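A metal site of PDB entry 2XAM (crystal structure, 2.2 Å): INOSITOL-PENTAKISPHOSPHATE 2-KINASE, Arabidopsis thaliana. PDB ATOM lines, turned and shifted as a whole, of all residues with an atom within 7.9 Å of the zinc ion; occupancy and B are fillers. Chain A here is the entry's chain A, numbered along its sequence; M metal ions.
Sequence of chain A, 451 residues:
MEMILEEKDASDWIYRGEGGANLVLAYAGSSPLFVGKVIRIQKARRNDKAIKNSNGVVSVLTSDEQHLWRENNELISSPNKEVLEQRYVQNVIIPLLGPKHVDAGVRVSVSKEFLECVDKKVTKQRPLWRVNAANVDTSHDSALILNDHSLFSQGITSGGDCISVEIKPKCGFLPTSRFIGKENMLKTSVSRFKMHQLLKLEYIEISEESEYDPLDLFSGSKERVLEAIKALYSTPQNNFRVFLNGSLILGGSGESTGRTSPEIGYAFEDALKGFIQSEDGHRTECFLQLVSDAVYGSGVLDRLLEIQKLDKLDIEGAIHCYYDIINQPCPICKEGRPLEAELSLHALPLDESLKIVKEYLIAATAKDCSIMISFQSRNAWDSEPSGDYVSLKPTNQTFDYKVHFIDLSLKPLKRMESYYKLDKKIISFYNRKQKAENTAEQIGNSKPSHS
The zinc ion is bound by NE2 of His 346, 1.9 Å away.
The zinc ion is bound by SG of Cys 330.
The zinc ion is bound by ND1 of His 320 (2.2 Å).
The zinc ion is bound by the side-chain sulfur (SG) of Cys 333 (2.4 Å).
The zinc ion has four donor atoms within binding distance.
Of the 18 residues printed, 4 come within 4 Å of the zinc ion.
The nearest printed residue that does not touch the zinc ion is Ile 332 (4.7 Å).
The side-chain sulfur (SG) of Cys 330 sits close to the backbone NH (N) of Ile 332.
ND1 of His 346 sits at hydrogen-bond distance from OD2 of Asp 324 (3.0 Å).
SG of Cys 333 lies close to N of Glu 342 (3.3 Å).
NE2 of His 320 sits close to O of Glu 316 (3.2 Å).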
ATOM      1  N   GLU A 316      -3.150  30.894   0.364  1.00  0.00           N
ATOM      2  CA  GLU A 316      -2.075  29.910   0.186  1.00  0.00           C
ATOM      3  C   GLU A 316      -0.830  30.333   0.951  1.00  0.00           C
ATOM      4  O   GLU A 316      -0.024  29.503   1.355  1.00  0.00           O
ATOM      5  CB  GLU A 316      -1.745  29.659  -1.280  1.00  0.00           C
ATOM      6  CG  GLU A 316      -2.877  29.020  -2.048  1.00  0.00           C
ATOM      7  CD  GLU A 316      -2.413  28.275  -3.278  1.00  0.00           C
ATOM      8  OE1 GLU A 316      -1.547  27.390  -3.122  1.00  0.00           O
ATOM      9  OE2 GLU A 316      -2.919  28.544  -4.377  1.00  0.00           O
ATOM     10  N   GLY A 317      -0.684  31.639   1.138  1.00  0.00           N
ATOM     11  CA  GLY A 317       0.387  32.180   1.936  1.00  0.00           C
ATOM     12  C   GLY A 317      -0.025  32.269   3.387  1.00  0.00           C
ATOM     13  O   GLY A 317       0.690  31.803   4.268  1.00  0.00           O
ATOM     14  N   ILE A 319      -2.208  30.776   5.230  1.00  0.00           N
ATOM     15  CA  ILE A 319      -2.417  29.526   5.947  1.00  0.00           C
ATOM     16  C   ILE A 319      -1.153  29.095   6.739  1.00  0.00           C
ATOM     17  O   ILE A 319      -1.254  28.572   7.856  1.00  0.00           O
ATOM     18  CB  ILE A 319      -2.859  28.379   4.990  1.00  0.00           C
ATOM     19  CG1 ILE A 319      -3.325  27.163   5.779  1.00  0.00           C
ATOM     20  CG2 ILE A 319      -1.754  28.001   4.056  1.00  0.00           C
ATOM     21  CD1 ILE A 319      -4.425  27.473   6.778  1.00  0.00           C
ATOM     22  N   HIS A 320       0.018  29.337   6.164  1.00  0.00           N
ATOM     23  CA  HIS A 320       1.259  28.974   6.858  1.00  0.00           C
ATOM     24  C   HIS A 320       1.423  29.685   8.204  1.00  0.00           C
ATOM     25  O   HIS A 320       1.760  29.063   9.202  1.00  0.00           O
ATOM     26  CB  HIS A 320       2.478  29.215   5.950  1.00  0.00           C
ATOM     27  CG  HIS A 320       2.464  28.405   4.698  1.00  0.00           C
ATOM     28  ND1 HIS A 320       3.041  27.157   4.599  1.00  0.00           N
ATOM     29  CD2 HIS A 320       1.916  28.662   3.479  1.00  0.00           C
ATOM     30  CE1 HIS A 320       2.863  26.678   3.386  1.00  0.00           C
ATOM     31  NE2 HIS A 320       2.184  27.566   2.683  1.00  0.00           N
ATOM     32  N   CYS A 321       1.190  31.000   8.221  1.00  0.00           N
ATOM     33  CA  CYS A 321       1.217  31.786   9.456  1.00  0.00           C
ATOM     34  C   CYS A 321       0.219  31.279  10.494  1.00  0.00           C
ATOM     35  O   CYS A 321       0.480  31.363  11.696  1.00  0.00           O
ATOM     36  CB  CYS A 321       0.894  33.245   9.137  1.00  0.00           C
ATOM     37  SG  CYS A 321       2.076  33.992   8.026  1.00  0.00           S
ATOM     38  N   TYR A 323      -0.831  28.160  11.120  1.00  0.00           N
ATOM     39  CA  TYR A 323      -0.321  27.025  11.869  1.00  0.00           C
ATOM     40  C   TYR A 323       0.759  27.456  12.878  1.00  0.00           C
ATOM     41  O   TYR A 323       0.850  26.891  13.964  1.00  0.00           O
ATOM     42  CB  TYR A 323       0.146  25.906  10.923  1.00  0.00           C
ATOM     43  CG  TYR A 323      -1.039  25.158  10.365  1.00  0.00           C
ATOM     44  CD1 TYR A 323      -1.778  24.295  11.161  1.00  0.00           C
ATOM     45  CD2 TYR A 323      -1.455  25.340   9.048  1.00  0.00           C
ATOM     46  CE1 TYR A 323      -2.877  23.628  10.678  1.00  0.00           C
ATOM     47  CE2 TYR A 323      -2.574  24.678   8.542  1.00  0.00           C
ATOM     48  CZ  TYR A 323      -3.275  23.823   9.360  1.00  0.00           C
ATOM     49  OH  TYR A 323      -4.374  23.156   8.877  1.00  0.00           O
ATOM     50  N   ASP A 324       1.537  28.474  12.535  1.00  0.00           N
ATOM     51  CA  ASP A 324       2.499  29.029  13.476  1.00  0.00           C
ATOM     52  C   ASP A 324       1.787  29.674  14.674  1.00  0.00           C
ATOM     53  O   ASP A 324       2.218  29.523  15.810  1.00  0.00           O
ATOM     54  CB  ASP A 324       3.398  30.068  12.780  1.00  0.00           C
ATOM     55  CG  ASP A 324       4.472  29.416  11.915  1.00  0.00           C
ATOM     56  OD1 ASP A 324       4.583  28.176  11.940  1.00  0.00           O
ATOM     57  OD2 ASP A 324       5.216  30.135  11.214  1.00  0.00           O
ATOM     58  N   GLN A 328       1.097  24.452  15.657  1.00  0.00           N
ATOM     59  CA  GLN A 328       1.070  23.110  15.124  1.00  0.00           C
ATOM     60  C   GLN A 328       2.061  23.017  13.983  1.00  0.00           C
ATOM     61  O   GLN A 328       2.234  23.989  13.238  1.00  0.00           O
ATOM     62  CB  GLN A 328      -0.324  22.726  14.617  1.00  0.00           C
ATOM     63  CG  GLN A 328      -0.281  21.596  13.580  1.00  0.00           C
ATOM     64  CD  GLN A 328      -1.653  21.234  13.034  1.00  0.00           C
ATOM     65  OE1 GLN A 328      -2.659  21.843  13.391  1.00  0.00           O
ATOM     66  NE2 GLN A 328      -1.688  20.236  12.146  1.00  0.00           N
ATOM     67  N   PRO A 329       2.717  21.864  13.840  1.00  0.00           N
ATOM     68  CA  PRO A 329       3.576  21.702  12.684  1.00  0.00           C
ATOM     69  C   PRO A 329       2.746  21.914  11.426  1.00  0.00           C
ATOM     70  O   PRO A 329       1.580  21.509  11.376  1.00  0.00           O
ATOM     71  CB  PRO A 329       4.067  20.253  12.786  1.00  0.00           C
ATOM     72  CG  PRO A 329       3.933  19.917  14.236  1.00  0.00           C
ATOM     73  CD  PRO A 329       2.716  20.664  14.698  1.00  0.00           C
ATOM     74  N   CYS A 330       3.336  22.577  10.439  1.00  0.00           N
ATOM     75  CA  CYS A 330       2.634  22.955   9.224  1.00  0.00           C
ATOM     76  C   CYS A 330       2.399  21.730   8.346  1.00  0.00           C
ATOM     77  O   CYS A 330       3.354  21.143   7.846  1.00  0.00           O
ATOM     78  CB  CYS A 330       3.454  23.996   8.458  1.00  0.00           C
ATOM     79  SG  CYS A 330       2.655  24.710   7.002  1.00  0.00           S
ATOM     80  N   PRO A 331       1.131  21.327   8.181  1.00  0.00           N
ATOM     81  CA  PRO A 331       0.793  20.160   7.363  1.00  0.00           C
ATOM     82  C   PRO A 331       0.864  20.461   5.871  1.00  0.00           C
ATOM     83  O   PRO A 331       0.893  19.534   5.067  1.00  0.00           O
ATOM     84  CB  PRO A 331      -0.645  19.858   7.766  1.00  0.00           C
ATOM     85  CG  PRO A 331      -1.203  21.182   8.181  1.00  0.00           C
ATOM     86  CD  PRO A 331      -0.063  21.922   8.823  1.00  0.00           C
ATOM     87  N   ILE A 332       0.896  21.736   5.507  1.00  0.00           N
ATOM     88  CA  ILE A 332       0.966  22.139   4.103  1.00  0.00           C
ATOM     89  C   ILE A 332       2.355  21.952   3.517  1.00  0.00           C
ATOM     90  O   ILE A 332       2.495  21.531   2.375  1.00  0.00           O
ATOM     91  CB  ILE A 332       0.548  23.600   3.914  1.00  0.00           C
ATOM     92  CG1 ILE A 332      -0.797  23.858   4.575  1.00  0.00           C
ATOM     93  CG2 ILE A 332       0.531  23.947   2.433  1.00  0.00           C
ATOM     94  CD1 ILE A 332      -1.900  22.922   4.120  1.00  0.00           C
ATOM     95  N   CYS A 333       3.382  22.272   4.301  1.00  0.00           N
ATOM     96  CA  CYS A 333       4.769  21.990   3.914  1.00  0.00           C
ATOM     97  C   CYS A 333       5.071  20.507   4.153  1.00  0.00           C
ATOM     98  O   CYS A 333       4.676  19.954   5.181  1.00  0.00           O
ATOM     99  CB  CYS A 333       5.739  22.882   4.705  1.00  0.00           C
ATOM    100  SG  CYS A 333       5.448  24.680   4.596  1.00  0.00           S
ATOM    101  N   LYS A 334       5.772  19.856   3.222  1.00  0.00           N
ATOM    102  CA  LYS A 334       6.031  18.415   3.359  1.00  0.00           C
ATOM    103  C   LYS A 334       7.504  18.057   3.476  1.00  0.00           C
ATOM    104  O   LYS A 334       8.384  18.930   3.450  1.00  0.00           O
ATOM    105  CB  LYS A 334       5.406  17.632   2.196  1.00  0.00           C
ATOM    106  CG  LYS A 334       3.889  17.528   2.261  1.00  0.00           C
ATOM    107  CD  LYS A 334       3.405  16.197   1.683  1.00  0.00           C
ATOM    108  CE  LYS A 334       1.943  15.943   2.037  1.00  0.00           C
ATOM    109  NZ  LYS A 334       1.402  14.729   1.370  1.00  0.00           N
ATOM    110  N   GLU A 342       7.900  26.729   3.619  1.00  0.00           N
ATOM    111  CA  GLU A 342       8.439  27.983   3.095  1.00  0.00           C
ATOM    112  C   GLU A 342       9.390  28.668   4.116  1.00  0.00           C
ATOM    113  O   GLU A 342       8.944  29.204   5.143  1.00  0.00           O
ATOM    114  CB  GLU A 342       7.311  28.929   2.701  1.00  0.00           C
ATOM    115  CG  GLU A 342       6.388  28.381   1.626  1.00  0.00           C
ATOM    116  CD  GLU A 342       5.280  29.360   1.259  1.00  0.00           C
ATOM    117  OE1 GLU A 342       5.237  30.456   1.841  1.00  0.00           O
ATOM    118  OE2 GLU A 342       4.449  29.013   0.387  1.00  0.00           O
ATOM    119  N   LEU A 343      10.720  28.640   3.806  1.00  0.00           N
ATOM    120  CA  LEU A 343      11.893  29.222   4.550  1.00  0.00           C
ATOM    121  C   LEU A 343      11.680  30.687   4.929  1.00  0.00           C
ATOM    122  O   LEU A 343      12.369  31.290   5.756  1.00  0.00           O
ATOM    123  CB  LEU A 343      13.119  29.225   3.596  1.00  0.00           C
ATOM    124  CG  LEU A 343      14.462  28.585   3.990  1.00  0.00           C
ATOM    125  CD1 LEU A 343      15.181  29.466   4.990  1.00  0.00           C
ATOM    126  CD2 LEU A 343      14.260  27.187   4.561  1.00  0.00           C
ATOM    127  N   LEU A 345       7.943  32.463   5.165  1.00  0.00           N
ATOM    128  CA  LEU A 345       6.845  32.814   6.069  1.00  0.00           C
ATOM    129  C   LEU A 345       7.029  32.231   7.470  1.00  0.00           C
ATOM    130  O   LEU A 345       6.718  32.869   8.469  1.00  0.00           O
ATOM    131  CB  LEU A 345       5.494  32.394   5.491  1.00  0.00           C
ATOM    132  CG  LEU A 345       4.999  33.088   4.217  1.00  0.00           C
ATOM    133  CD1 LEU A 345       3.637  32.539   3.829  1.00  0.00           C
ATOM    134  CD2 LEU A 345       4.946  34.590   4.409  1.00  0.00           C
ATOM    135  N   HIS A 346       7.550  31.006   7.531  1.00  0.00           N
ATOM    136  CA  HIS A 346       7.712  30.337   8.813  1.00  0.00           C
ATOM    137  C   HIS A 346       8.856  30.930   9.649  1.00  0.00           C
ATOM    138  O   HIS A 346       9.004  30.575  10.821  1.00  0.00           O
ATOM    139  CB  HIS A 346       7.872  28.833   8.630  1.00  0.00           C
ATOM    140  CG  HIS A 346       6.602  28.127   8.233  1.00  0.00           C
ATOM    141  ND1 HIS A 346       5.493  28.106   9.050  1.00  0.00           N
ATOM    142  CD2 HIS A 346       6.284  27.417   7.129  1.00  0.00           C
ATOM    143  CE1 HIS A 346       4.533  27.415   8.454  1.00  0.00           C
ATOM    144  NE2 HIS A 346       4.982  27.003   7.286  1.00  0.00           N
HETATM  145 ZN    ZN M   1       4.003  25.869   6.056  1.00  0.00          ZN
